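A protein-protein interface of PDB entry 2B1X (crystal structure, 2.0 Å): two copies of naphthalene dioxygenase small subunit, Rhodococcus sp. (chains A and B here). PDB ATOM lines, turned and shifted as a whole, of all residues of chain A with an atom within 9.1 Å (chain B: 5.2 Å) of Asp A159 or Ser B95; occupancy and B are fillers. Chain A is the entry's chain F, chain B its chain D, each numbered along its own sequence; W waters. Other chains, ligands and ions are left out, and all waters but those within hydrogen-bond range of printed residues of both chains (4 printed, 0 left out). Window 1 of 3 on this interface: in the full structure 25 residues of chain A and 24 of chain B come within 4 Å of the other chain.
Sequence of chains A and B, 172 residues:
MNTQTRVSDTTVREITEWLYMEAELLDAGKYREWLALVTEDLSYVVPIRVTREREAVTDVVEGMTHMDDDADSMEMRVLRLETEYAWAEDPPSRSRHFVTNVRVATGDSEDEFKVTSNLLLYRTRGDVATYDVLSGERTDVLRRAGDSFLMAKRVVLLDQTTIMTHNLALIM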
ATOM      1  N   VAL A  46       6.742 -23.913  -5.576  1.00  0.00           N
ATOM      2  CA  VAL A  46       8.129 -23.530  -5.904  1.00  0.00           C
ATOM      3  C   VAL A  46       8.866 -24.862  -5.990  1.00  0.00           C
ATOM      4  O   VAL A  46       9.218 -25.407  -4.968  1.00  0.00           O
ATOM      5  CB  VAL A  46       8.757 -22.655  -4.779  1.00  0.00           C
ATOM      6  CG1 VAL A  46      10.206 -22.184  -5.178  1.00  0.00           C
ATOM      7  CG2 VAL A  46       7.916 -21.411  -4.493  1.00  0.00           C
ATOM      8  N   PRO A  47       9.042 -25.413  -7.188  1.00  0.00           N
ATOM      9  CA  PRO A  47       9.728 -26.705  -7.354  1.00  0.00           C
ATOM     10  C   PRO A  47      11.231 -26.670  -7.096  1.00  0.00           C
ATOM     11  O   PRO A  47      11.857 -25.614  -7.154  1.00  0.00           O
ATOM     12  CB  PRO A  47       9.467 -27.061  -8.840  1.00  0.00           C
ATOM     13  CG  PRO A  47       8.326 -26.130  -9.265  1.00  0.00           C
ATOM     14  CD  PRO A  47       8.548 -24.872  -8.470  1.00  0.00           C
ATOM     15  N   ARG A  49      14.932 -27.887  -8.406  1.00  0.00           N
ATOM     16  CA  ARG A  49      15.655 -28.301  -9.607  1.00  0.00           C
ATOM     17  C   ARG A  49      17.023 -28.857  -9.238  1.00  0.00           C
ATOM     18  O   ARG A  49      17.609 -28.482  -8.217  1.00  0.00           O
ATOM     19  CB  ARG A  49      15.845 -27.110 -10.555  1.00  0.00           C
ATOM     20  CG  ARG A  49      14.523 -26.535 -11.078  1.00  0.00           C
ATOM     21  CD  ARG A  49      14.734 -25.314 -11.985  1.00  0.00           C
ATOM     22  NE  ARG A  49      15.392 -25.693 -13.229  1.00  0.00           N
ATOM     23  CZ  ARG A  49      15.688 -24.883 -14.201  1.00  0.00           C
ATOM     24  NH1 ARG A  49      15.395 -23.580 -14.090  1.00  0.00           N
ATOM     25  NH2 ARG A  49      16.277 -25.369 -15.296  1.00  0.00           N
ATOM     26  N   ARG A  54      21.961 -32.239 -20.666  1.00  0.00           N
ATOM     27  CA  ARG A  54      21.004 -31.627 -21.583  1.00  0.00           C
ATOM     28  C   ARG A  54      19.948 -32.652 -22.046  1.00  0.00           C
ATOM     29  O   ARG A  54      18.781 -32.312 -22.232  1.00  0.00           O
ATOM     30  CB  ARG A  54      21.773 -31.014 -22.770  1.00  0.00           C
ATOM     31  CG  ARG A  54      20.953 -30.268 -23.788  1.00  0.00           C
ATOM     32  CD  ARG A  54      21.733 -29.166 -24.531  1.00  0.00           C
ATOM     33  NE  ARG A  54      20.950 -27.947 -24.414  1.00  0.00           N
ATOM     34  CZ  ARG A  54      21.365 -26.776 -23.986  1.00  0.00           C
ATOM     35  NH1 ARG A  54      22.616 -26.549 -23.631  1.00  0.00           N
ATOM     36  NH2 ARG A  54      20.479 -25.797 -23.935  1.00  0.00           N
ATOM     37  N   ASP A  59      14.636 -31.388 -15.396  1.00  0.00           N
ATOM     38  CA  ASP A  59      15.523 -31.263 -14.245  1.00  0.00           C
ATOM     39  C   ASP A  59      14.731 -30.884 -12.990  1.00  0.00           C
ATOM     40  O   ASP A  59      15.331 -30.583 -11.950  1.00  0.00           O
ATOM     41  CB  ASP A  59      16.697 -30.284 -14.516  1.00  0.00           C
ATOM     42  CG  ASP A  59      16.251 -28.843 -14.805  1.00  0.00           C
ATOM     43  OD1 ASP A  59      15.063 -28.483 -14.554  1.00  0.00           O
ATOM     44  OD2 ASP A  59      17.034 -27.982 -15.296  1.00  0.00           O
ATOM     45  N   SER A 117       5.562 -14.426 -16.395  1.00  0.00           N
ATOM     46  CA  SER A 117       6.388 -13.239 -16.173  1.00  0.00           C
ATOM     47  C   SER A 117       7.746 -13.628 -15.625  1.00  0.00           C
ATOM     48  O   SER A 117       7.878 -14.646 -14.975  1.00  0.00           O
ATOM     49  CB  SER A 117       5.666 -12.231 -15.253  1.00  0.00           C
ATOM     50  OG  SER A 117       5.237 -12.809 -14.005  1.00  0.00           O
ATOM     51  N   ASN A 118       8.766 -12.827 -15.915  1.00  0.00           N
ATOM     52  CA  ASN A 118      10.078 -13.044 -15.325  1.00  0.00           C
ATOM     53  C   ASN A 118      10.136 -12.249 -14.018  1.00  0.00           C
ATOM     54  O   ASN A 118       9.651 -11.115 -13.947  1.00  0.00           O
ATOM     55  CB  ASN A 118      11.183 -12.598 -16.289  1.00  0.00           C
ATOM     56  CG  ASN A 118      11.413 -13.593 -17.423  1.00  0.00           C
ATOM     57  OD1 ASN A 118      10.873 -14.709 -17.405  1.00  0.00           O
ATOM     58  ND2 ASN A 118      12.238 -13.211 -18.396  1.00  0.00           N
ATOM     59  N   LEU A 119      10.718 -12.862 -12.996  1.00  0.00           N
ATOM     60  CA  LEU A 119      10.841 -12.253 -11.683  1.00  0.00           C
ATOM     61  C   LEU A 119      12.289 -12.167 -11.287  1.00  0.00           C
ATOM     62  O   LEU A 119      13.032 -13.171 -11.363  1.00  0.00           O
ATOM     63  CB  LEU A 119      10.056 -13.063 -10.627  1.00  0.00           C
ATOM     64  CG  LEU A 119      10.302 -12.642  -9.156  1.00  0.00           C
ATOM     65  CD1 LEU A 119       9.653 -11.261  -8.803  1.00  0.00           C
ATOM     66  CD2 LEU A 119       9.831 -13.699  -8.157  1.00  0.00           C
ATOM     67  N   LEU A 120      12.714 -10.982 -10.884  1.00  0.00           N
ATOM     68  CA  LEU A 120      13.967 -10.894 -10.178  1.00  0.00           C
ATOM     69  C   LEU A 120      13.630 -10.317  -8.838  1.00  0.00           C
ATOM     70  O   LEU A 120      13.090  -9.211  -8.744  1.00  0.00           O
ATOM     71  CB  LEU A 120      14.971 -10.020 -10.931  1.00  0.00           C
ATOM     72  CG  LEU A 120      16.267  -9.346 -10.444  1.00  0.00           C
ATOM     73  CD1 LEU A 120      16.550  -9.264  -8.921  1.00  0.00           C
ATOM     74  CD2 LEU A 120      17.449  -9.876 -11.213  1.00  0.00           C
ATOM     75  N   LEU A 121      13.923 -11.075  -7.806  1.00  0.00           N
ATOM     76  CA  LEU A 121      13.624 -10.642  -6.443  1.00  0.00           C
ATOM     77  C   LEU A 121      14.876 -10.222  -5.726  1.00  0.00           C
ATOM     78  O   LEU A 121      15.807 -11.025  -5.555  1.00  0.00           O
ATOM     79  CB  LEU A 121      12.929 -11.757  -5.663  1.00  0.00           C
ATOM     80  CG  LEU A 121      12.574 -11.465  -4.200  1.00  0.00           C
ATOM     81  CD1 LEU A 121      11.450 -10.451  -4.096  1.00  0.00           C
ATOM     82  CD2 LEU A 121      12.212 -12.767  -3.470  1.00  0.00           C
ATOM     83  N   VAL A 133      19.774 -12.202  -4.484  1.00  0.00           N
ATOM     84  CA  VAL A 133      18.942 -12.087  -5.694  1.00  0.00           C
ATOM     85  C   VAL A 133      18.332 -13.457  -5.971  1.00  0.00           C
ATOM     86  O   VAL A 133      19.047 -14.476  -6.033  1.00  0.00           O
ATOM     87  CB  VAL A 133      19.794 -11.657  -6.921  1.00  0.00           C
ATOM     88  CG1 VAL A 133      18.927 -11.679  -8.216  1.00  0.00           C
ATOM     89  CG2 VAL A 133      20.337 -10.275  -6.729  1.00  0.00           C
ATOM     90  N   LEU A 134      17.025 -13.526  -6.094  1.00  0.00           N
ATOM     91  CA  LEU A 134      16.402 -14.715  -6.701  1.00  0.00           C
ATOM     92  C   LEU A 134      15.960 -14.325  -8.109  1.00  0.00           C
ATOM     93  O   LEU A 134      15.435 -13.214  -8.345  1.00  0.00           O
ATOM     94  CB  LEU A 134      15.205 -15.208  -5.885  1.00  0.00           C
ATOM     95  CG  LEU A 134      15.478 -15.617  -4.428  1.00  0.00           C
ATOM     96  CD1 LEU A 134      14.161 -16.159  -3.801  1.00  0.00           C
ATOM     97  CD2 LEU A 134      16.558 -16.705  -4.409  1.00  0.00           C
ATOM     98  N   SER A 135      16.160 -15.232  -9.049  1.00  0.00           N
ATOM     99  CA  SER A 135      15.696 -15.011 -10.425  1.00  0.00           C
ATOM    100  C   SER A 135      14.845 -16.218 -10.804  1.00  0.00           C
ATOM    101  O   SER A 135      15.174 -17.339 -10.412  1.00  0.00           O
ATOM    102  CB  SER A 135      16.867 -14.899 -11.391  1.00  0.00           C
ATOM    103  OG  SER A 135      16.402 -15.046 -12.719  1.00  0.00           O
ATOM    104  N   GLY A 136      13.785 -15.991 -11.562  1.00  0.00           N
ATOM    105  CA  GLY A 136      12.932 -17.102 -11.933  1.00  0.00           C
ATOM    106  C   GLY A 136      11.807 -16.744 -12.882  1.00  0.00           C
ATOM    107  O   GLY A 136      11.608 -15.548 -13.235  1.00  0.00           O
ATOM    108  N   GLU A 137      11.073 -17.773 -13.312  1.00  0.00           N
ATOM    109  CA  GLU A 137       9.889 -17.552 -14.133  1.00  0.00           C
ATOM    110  C   GLU A 137       8.635 -17.972 -13.369  1.00  0.00           C
ATOM    111  O   GLU A 137       8.565 -19.079 -12.826  1.00  0.00           O
ATOM    112  CB  GLU A 137       9.967 -18.329 -15.442  1.00  0.00           C
ATOM    113  CG  GLU A 137       8.794 -18.034 -16.375  1.00  0.00           C
ATOM    114  CD  GLU A 137       8.989 -18.583 -17.785  1.00  0.00           C
ATOM    115  OE1 GLU A 137       8.970 -19.820 -17.954  1.00  0.00           O
ATOM    116  OE2 GLU A 137       9.133 -17.781 -18.732  1.00  0.00           O
ATOM    117  N   ARG A 138       7.652 -17.091 -13.348  1.00  0.00           N
ATOM    118  CA  ARG A 138       6.365 -17.401 -12.731  1.00  0.00           C
ATOM    119  C   ARG A 138       5.358 -17.736 -13.824  1.00  0.00           C
ATOM    120  O   ARG A 138       5.196 -16.985 -14.792  1.00  0.00           O
ATOM    121  CB  ARG A 138       5.875 -16.210 -11.897  1.00  0.00           C
ATOM    122  CG  ARG A 138       6.891 -15.706 -10.869  1.00  0.00           C
ATOM    123  CD  ARG A 138       6.380 -14.518 -10.004  1.00  0.00           C
ATOM    124  NE  ARG A 138       5.801 -13.448 -10.813  1.00  0.00           N
ATOM    125  CZ  ARG A 138       5.230 -12.343 -10.310  1.00  0.00           C
ATOM    126  NH1 ARG A 138       5.191 -12.121  -8.996  1.00  0.00           N
ATOM    127  NH2 ARG A 138       4.679 -11.454 -11.126  1.00  0.00           N
ATOM    128  N   VAL A 156       6.473 -20.912  -9.346  1.00  0.00           N
ATOM    129  CA  VAL A 156       7.719 -20.118  -9.406  1.00  0.00           C
ATOM    130  C   VAL A 156       8.894 -21.028  -9.644  1.00  0.00           C
ATOM    131  O   VAL A 156       9.330 -21.703  -8.731  1.00  0.00           O
ATOM    132  CB  VAL A 156       7.984 -19.334  -8.129  1.00  0.00           C
ATOM    133  CG1 VAL A 156       9.168 -18.370  -8.351  1.00  0.00           C
ATOM    134  CG2 VAL A 156       6.740 -18.492  -7.780  1.00  0.00           C
ATOM    135  N   LEU A 157       9.408 -21.021 -10.864  1.00  0.00           N
ATOM    136  CA  LEU A 157      10.527 -21.894 -11.234  1.00  0.00           C
ATOM    137  C   LEU A 157      11.798 -21.054 -11.198  1.00  0.00           C
ATOM    138  O   LEU A 157      12.026 -20.247 -12.094  1.00  0.00           O
ATOM    139  CB  LEU A 157      10.323 -22.472 -12.631  1.00  0.00           C
ATOM    140  CG  LEU A 157      11.080 -23.792 -12.952  1.00  0.00           C
ATOM    141  CD1 LEU A 157      10.863 -24.851 -11.889  1.00  0.00           C
ATOM    142  CD2 LEU A 157      10.621 -24.351 -14.313  1.00  0.00           C
ATOM    143  N   LEU A 158      12.625 -21.247 -10.175  1.00  0.00           N
ATOM    144  CA  LEU A 158      13.821 -20.434 -10.025  1.00  0.00           C
ATOM    145  C   LEU A 158      14.969 -20.935 -10.881  1.00  0.00           C
ATOM    146  O   LEU A 158      15.127 -22.151 -11.101  1.00  0.00           O
ATOM    147  CB  LEU A 158      14.267 -20.381  -8.560  1.00  0.00           C
ATOM    148  CG  LEU A 158      13.226 -19.853  -7.587  1.00  0.00           C
ATOM    149  CD1 LEU A 158      13.733 -20.158  -6.145  1.00  0.00           C
ATOM    150  CD2 LEU A 158      12.973 -18.387  -7.784  1.00  0.00           C
ATOM    151  N   ASP A 159      15.814 -19.999 -11.308  1.00  0.00           N
ATOM    152  CA  ASP A 159      16.993 -20.330 -12.128  1.00  0.00           C
ATOM    153  C   ASP A 159      18.168 -20.712 -11.258  1.00  0.00           C
ATOM    154  O   ASP A 159      19.289 -20.184 -11.427  1.00  0.00           O
ATOM    155  CB  ASP A 159      17.359 -19.125 -12.993  1.00  0.00           C
ATOM    156  CG  ASP A 159      16.198 -18.685 -13.861  1.00  0.00           C
ATOM    157  OD1 ASP A 159      15.686 -19.558 -14.626  1.00  0.00           O
ATOM    158  OD2 ASP A 159      15.688 -17.529 -13.821  1.00  0.00           O
ATOM    159  N   GLN A 160      17.888 -21.592 -10.291  1.00  0.00           N
ATOM    160  CA  GLN A 160      18.852 -22.025  -9.273  1.00  0.00           C
ATOM    161  C   GLN A 160      18.551 -23.457  -8.914  1.00  0.00           C
ATOM    162  O   GLN A 160      17.397 -23.917  -9.062  1.00  0.00           O
ATOM    163  CB  GLN A 160      18.759 -21.154  -7.993  1.00  0.00           C
ATOM    164  CG  GLN A 160      19.105 -19.676  -8.200  1.00  0.00           C
ATOM    165  CD  GLN A 160      18.814 -18.776  -6.992  1.00  0.00           C
ATOM    166  OE1 GLN A 160      18.518 -19.252  -5.888  1.00  0.00           O
ATOM    167  NE2 GLN A 160      18.908 -17.477  -7.203  1.00  0.00           N
ATOM    168  N   THR A 161      19.581 -24.189  -8.464  1.00  0.00           N
ATOM    169  CA  THR A 161      19.341 -25.502  -7.903  1.00  0.00           C
ATOM    170  C   THR A 161      19.467 -25.301  -6.378  1.00  0.00           C
ATOM    171  O   THR A 161      18.458 -25.317  -5.675  1.00  0.00           O
ATOM    172  CB  THR A 161      20.268 -26.596  -8.523  1.00  0.00           C
ATOM    173  OG1 THR A 161      21.657 -26.194  -8.463  1.00  0.00           O
ATOM    174  CG2 THR A 161      19.963 -26.789 -10.070  1.00  0.00           C
ATOM    175  N   THR A 162      20.680 -25.006  -5.926  1.00  0.00           N
ATOM    176  CA  THR A 162      21.000 -24.532  -4.573  1.00  0.00           C
ATOM    177  C   THR A 162      20.506 -23.080  -4.456  1.00  0.00           C
ATOM    178  O   THR A 162      20.921 -22.187  -5.253  1.00  0.00           O
ATOM    179  CB  THR A 162      22.524 -24.650  -4.352  1.00  0.00           C
ATOM    180  OG1 THR A 162      22.907 -26.051  -4.443  1.00  0.00           O
ATOM    181  CG2 THR A 162      22.924 -24.275  -2.898  1.00  0.00           C
ATOM    182  N   ILE A 163      19.584 -22.853  -3.527  1.00  0.00           N
ATOM    183  CA  ILE A 163      18.918 -21.558  -3.451  1.00  0.00           C
ATOM    184  C   ILE A 163      19.826 -20.583  -2.732  1.00  0.00           C
ATOM    185  O   ILE A 163      20.462 -20.928  -1.705  1.00  0.00           O
ATOM    186  CB  ILE A 163      17.537 -21.665  -2.764  1.00  0.00           C
ATOM    187  CG1 ILE A 163      16.657 -22.731  -3.462  1.00  0.00           C
ATOM    188  CG2 ILE A 163      16.822 -20.231  -2.699  1.00  0.00           C
ATOM    189  CD1 ILE A 163      16.449 -22.528  -4.996  1.00  0.00           C
ATOM    190  N   MET A 164      19.920 -19.362  -3.277  1.00  0.00           N
ATOM    191  CA  MET A 164      20.877 -18.399  -2.752  1.00  0.00           C
ATOM    192  C   MET A 164      20.248 -17.305  -1.893  1.00  0.00           C
ATOM    193  O   MET A 164      20.492 -16.134  -2.076  1.00  0.00           O
ATOM    194  CB  MET A 164      21.762 -17.847  -3.884  1.00  0.00           C
ATOM    195  CG  MET A 164      22.735 -18.944  -4.387  1.00  0.00           C
ATOM    196  SD  MET A 164      23.783 -18.464  -5.703  1.00  0.00           S
ATOM    197  CE  MET A 164      22.666 -18.732  -7.091  1.00  0.00           C
ATOM    198  N   LEU B  26      15.194 -18.728 -25.881  1.00  0.00           N
ATOM    199  CA  LEU B  26      16.570 -18.807 -25.370  1.00  0.00           C
ATOM    200  C   LEU B  26      16.663 -19.399 -23.965  1.00  0.00           C
ATOM    201  O   LEU B  26      17.490 -20.253 -23.718  1.00  0.00           O
ATOM    202  CB  LEU B  26      17.219 -17.440 -25.386  1.00  0.00           C
ATOM    203  CG  LEU B  26      18.021 -16.984 -26.617  1.00  0.00           C
ATOM    204  CD1 LEU B  26      18.133 -17.972 -27.734  1.00  0.00           C
ATOM    205  CD2 LEU B  26      17.573 -15.600 -27.102  1.00  0.00           C
ATOM    206  N   ASP B  27      15.811 -18.929 -23.061  1.00  0.00           N
ATOM    207  CA  ASP B  27      15.800 -19.414 -21.691  1.00  0.00           C
ATOM    208  C   ASP B  27      15.286 -20.858 -21.567  1.00  0.00           C
ATOM    209  O   ASP B  27      15.456 -21.504 -20.515  1.00  0.00           O
ATOM    210  CB  ASP B  27      14.990 -18.457 -20.817  1.00  0.00           C
ATOM    211  CG  ASP B  27      15.659 -17.095 -20.665  1.00  0.00           C
ATOM    212  OD1 ASP B  27      16.906 -17.019 -20.796  1.00  0.00           O
ATOM    213  OD2 ASP B  27      15.009 -16.031 -20.423  1.00  0.00           O
ATOM    214  N   SER B  93      23.393 -24.178 -18.602  1.00  0.00           N
ATOM    215  CA  SER B  93      23.215 -23.096 -17.643  1.00  0.00           C
ATOM    216  C   SER B  93      21.714 -22.929 -17.380  1.00  0.00           C
ATOM    217  O   SER B  93      20.896 -23.234 -18.228  1.00  0.00           O
ATOM    218  CB  SER B  93      23.760 -21.795 -18.243  1.00  0.00           C
ATOM    219  OG  SER B  93      25.161 -21.903 -18.431  1.00  0.00           O
ATOM    220  N   ARG B  94      21.360 -22.406 -16.219  1.00  0.00           N
ATOM    221  CA  ARG B  94      20.036 -21.851 -16.032  1.00  0.00           C
ATOM    222  C   ARG B  94      20.197 -20.376 -16.313  1.00  0.00           C
ATOM    223  O   ARG B  94      21.057 -19.726 -15.717  1.00  0.00           O
ATOM    224  CB  ARG B  94      19.565 -22.026 -14.586  1.00  0.00           C
ATOM    225  CG  ARG B  94      18.963 -23.359 -14.342  1.00  0.00           C
ATOM    226  CD  ARG B  94      20.016 -24.395 -14.023  1.00  0.00           C
ATOM    227  NE  ARG B  94      20.970 -23.912 -12.994  1.00  0.00           N
ATOM    228  CZ  ARG B  94      21.906 -24.679 -12.438  1.00  0.00           C
ATOM    229  NH1 ARG B  94      22.003 -25.968 -12.813  1.00  0.00           N
ATOM    230  NH2 ARG B  94      22.729 -24.176 -11.496  1.00  0.00           N
ATOM    231  N   SER B  95      19.378 -19.840 -17.202  1.00  0.00           N
ATOM    232  CA  SER B  95      19.497 -18.433 -17.553  1.00  0.00           C
ATOM    233  C   SER B  95      18.160 -17.711 -17.564  1.00  0.00           C
ATOM    234  O   SER B  95      17.105 -18.330 -17.744  1.00  0.00           O
ATOM    235  CB  SER B  95      20.153 -18.297 -18.923  1.00  0.00           C
ATOM    236  OG  SER B  95      19.263 -18.734 -19.940  1.00  0.00           O
ATOM    237  N   ARG B  96      18.205 -16.387 -17.415  1.00  0.00           N
ATOM    238  CA  ARG B  96      17.026 -15.564 -17.586  1.00  0.00           C
ATOM    239  C   ARG B  96      17.428 -14.282 -18.284  1.00  0.00           C
ATOM    240  O   ARG B  96      18.363 -13.578 -17.846  1.00  0.00           O
ATOM    241  CB  ARG B  96      16.343 -15.245 -16.255  1.00  0.00           C
ATOM    242  CG  ARG B  96      14.881 -14.722 -16.432  1.00  0.00           C
ATOM    243  CD  ARG B  96      13.844 -15.419 -15.511  1.00  0.00           C
ATOM    244  NE  ARG B  96      13.996 -16.871 -15.696  1.00  0.00           N
ATOM    245  CZ  ARG B  96      13.450 -17.577 -16.682  1.00  0.00           C
ATOM    246  NH1 ARG B  96      12.610 -16.980 -17.571  1.00  0.00           N
ATOM    247  NH2 ARG B  96      13.760 -18.888 -16.803  1.00  0.00           N
ATOM    248  N   HIS B  97      16.724 -14.027 -19.388  1.00  0.00           N
ATOM    249  CA  HIS B  97      16.855 -12.817 -20.150  1.00  0.00           C
ATOM    250  C   HIS B  97      15.764 -11.854 -19.668  1.00  0.00           C
ATOM    251  O   HIS B  97      14.589 -11.984 -20.080  1.00  0.00           O
ATOM    252  CB  HIS B  97      16.623 -13.102 -21.658  1.00  0.00           C
ATOM    253  CG  HIS B  97      17.755 -13.799 -22.340  1.00  0.00           C
ATOM    254  ND1 HIS B  97      18.117 -15.105 -22.048  1.00  0.00           N
ATOM    255  CD2 HIS B  97      18.594 -13.385 -23.327  1.00  0.00           C
ATOM    256  CE1 HIS B  97      19.146 -15.449 -22.806  1.00  0.00           C
ATOM    257  NE2 HIS B  97      19.444 -14.433 -23.601  1.00  0.00           N
ATOM    258  N   LEU B 121      21.069 -10.343 -18.033  1.00  0.00           N
ATOM    259  CA  LEU B 121      21.114 -11.798 -18.202  1.00  0.00           C
ATOM    260  C   LEU B 121      21.641 -12.404 -16.915  1.00  0.00           C
ATOM    261  O   LEU B 121      22.748 -12.064 -16.470  1.00  0.00           O
ATOM    262  CB  LEU B 121      22.006 -12.150 -19.370  1.00  0.00           C
ATOM    263  CG  LEU B 121      22.242 -13.627 -19.659  1.00  0.00           C
ATOM    264  CD1 LEU B 121      20.914 -14.319 -20.110  1.00  0.00           C
ATOM    265  CD2 LEU B 121      23.321 -13.745 -20.717  1.00  0.00           C
ATOM    266  N   TYR B 122      20.847 -13.282 -16.319  1.00  0.00           N
ATOM    267  CA  TYR B 122      21.209 -13.980 -15.098  1.00  0.00           C
ATOM    268  C   TYR B 122      21.661 -15.399 -15.489  1.00  0.00           C
ATOM    269  O   TYR B 122      21.057 -16.019 -16.349  1.00  0.00           O
ATOM    270  CB  TYR B 122      19.968 -14.060 -14.198  1.00  0.00           C
ATOM    271  CG  TYR B 122      20.184 -14.736 -12.866  1.00  0.00           C
ATOM    272  CD1 TYR B 122      20.600 -14.002 -11.747  1.00  0.00           C
ATOM    273  CD2 TYR B 122      20.001 -16.104 -12.737  1.00  0.00           C
ATOM    274  CE1 TYR B 122      20.787 -14.628 -10.514  1.00  0.00           C
ATOM    275  CE2 TYR B 122      20.187 -16.743 -11.540  1.00  0.00           C
ATOM    276  CZ  TYR B 122      20.590 -16.003 -10.424  1.00  0.00           C
ATOM    277  OH  TYR B 122      20.779 -16.622  -9.225  1.00  0.00           O
ATOM    278  N   ARG B 123      22.718 -15.907 -14.854  1.00  0.00           N
ATOM    279  CA  ARG B 123      23.246 -17.226 -15.209  1.00  0.00           C
ATOM    280  C   ARG B 123      23.782 -18.002 -14.016  1.00  0.00           C
ATOM    281  O   ARG B 123      24.580 -17.461 -13.239  1.00  0.00           O
ATOM    282  CB  ARG B 123      24.322 -17.092 -16.299  1.00  0.00           C
ATOM    283  CG  ARG B 123      24.989 -18.421 -16.709  1.00  0.00           C
ATOM    284  CD  ARG B 123      26.340 -18.226 -17.452  1.00  0.00           C
ATOM    285  NE  ARG B 123      26.679 -19.380 -18.319  1.00  0.00           N
ATOM    286  CZ  ARG B 123      27.771 -19.459 -19.120  1.00  0.00           C
ATOM    287  NH1 ARG B 123      28.668 -18.471 -19.151  1.00  0.00           N
ATOM    288  NH2 ARG B 123      27.962 -20.525 -19.911  1.00  0.00           N
ATOM    289  N   THR B 124      23.310 -19.244 -13.837  1.00  0.00           N
ATOM    290  CA  THR B 124      23.982 -20.197 -12.897  1.00  0.00           C
ATOM    291  C   THR B 124      24.327 -21.494 -13.565  1.00  0.00           C
ATOM    292  O   THR B 124      23.694 -21.893 -14.555  1.00  0.00           O
ATOM    293  CB  THR B 124      23.128 -20.506 -11.629  1.00  0.00           C
ATOM    294  OG1 THR B 124      21.897 -21.143 -12.025  1.00  0.00           O
ATOM    295  CG2 THR B 124      22.703 -19.224 -10.909  1.00  0.00           C
ATOM    296  N   LEU B 170      26.186 -18.444 -24.109  1.00  0.00           N
ATOM    297  CA  LEU B 170      24.744 -18.151 -24.235  1.00  0.00           C
ATOM    298  C   LEU B 170      24.474 -17.036 -25.236  1.00  0.00           C
ATOM    299  O   LEU B 170      25.197 -16.031 -25.272  1.00  0.00           O
ATOM    300  CB  LEU B 170      24.141 -17.753 -22.866  1.00  0.00           C
ATOM    301  CG  LEU B 170      24.210 -18.749 -21.709  1.00  0.00           C
ATOM    302  CD1 LEU B 170      23.705 -18.066 -20.406  1.00  0.00           C
ATOM    303  CD2 LEU B 170      23.383 -19.967 -22.024  1.00  0.00           C
HETATM  304  O   HOH W   1      13.421 -21.164 -14.176  1.00  0.00           O
HETATM  305  O   HOH W   2      21.256 -15.300  -7.054  1.00  0.00           O
HETATM  306  O   HOH W   3      12.353 -15.433 -20.638  1.00  0.00           O
HETATM  307  O   HOH W   4      11.255 -17.995 -19.977  1.00  0.00           O
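The backbone NH (N) of Arg B94 is in hydrogen-bond range of the backbone carbonyl oxygen (O) of Thr B124 (2.9 Å).
The backbone NH (N) of Leu A119 is in hydrogen-bond range of the backbone carbonyl oxygen (O) of Gly A136 (2.8 Å).
Water W4 lies within hydrogen-bond range of the side-chain carboxylate of Glu A137 (2.5 Å) and the guanidinium group of Arg B96 (2.9 Å).
Water W1 lies within hydrogen-bond range of O of Leu A157 (2.7 Å), OD1 of Asp A159 (2.8 Å), NH1 of Arg A49 (3.1 Å) and NH2 of Arg B96 (3.5 Å).
Asp A159 touches five residues of chain B.
No residue of chain A comes within 4 Å of Asp B27.
Of chain A, only Asn A118, Ser A135, Gly A136, Glu A137 and Asp A159 come within 4 Å of Arg B96.
Printed residues of chain A within 4 Å of Arg B94: Arg A49 (3.5 Å), Asp A159 (3.7 Å) and Thr A161 (3.5 Å).
Of the printed residues of chain A, Tyr B122 touches Ser A135, Asp A159, Gln A160 and Met A164.
Val A133 touches none of the printed residues of chain B.
The nearest printed residue of chain B that does not touch Asp A159 is Arg B123 (5.6 Å).
Ser A135 touches Arg B96.
CB of Ser A135 touches CD2 of Tyr B122, 3.6 Å away.
Gly A136 touches Arg B96 (O to CD, 3.2 Å).
Asp A159 touches Arg B94.
Tyr B122 touches Asp A159.
NH1 of Arg B94 touches CG2 of Thr A161, at 3.5 Å.
Met A164 touches Tyr B122.
CG2 of Thr B124 touches CE of Met A164 (3.8 Å).
Of the 12 printed residues of chain B, 6 touch a printed residue of chain A.
Of the 25 printed residues of chain A, 9 touch a printed residue of chain B.
Hydrophobic or aromatic side chains of chain A within 4 Å of the printed part of chain B: Met A164.
Along chain A the printed residues that touch a printed residue of chain B span positions 49 to 164.
Among the printed residues, 16 pairs touch across the chains.
Among the printed residues, Asp or Glu carboxylates within 4 Å of a Lys or Arg side-chain nitrogen of the other chain: Glu A137 with Arg B96 (3.8 Å) and Asp A159 with Arg B96 (2.6 Å).
The side-chain amide oxygen (OD1) of Asn A118 is in hydrogen-bond range of the guanidinium group (NH1) of Arg B96, at 2.9 Å.
NH1 of Arg B96 is in salt-bridge range of OE2 of Glu A137 (3.8 Å).
The side-chain carboxylate (OD2) of Asp A159 is in salt-bridge range of the guanidinium group (NE) of Arg B96, at 2.6 Å.
The side-chain amide nitrogen (ND2) of Asn A118 is in hydrogen-bond range of the backbone carbonyl oxygen (O) of His B97 (3.1 Å).
The side-chain amide nitrogen (NE2) of Gln A160 is in hydrogen-bond range of the side-chain hydroxyl (OH) of Tyr B122 (2.9 Å).
OG1 of Thr B124 lies within hydrogen-bond range of O of Asp A159, at 2.8 Å.
1 position is printed for both chains.
Of the 16 pairs that touch across the chains among the printed residues, none has its exchanged pair printed and touching as well.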
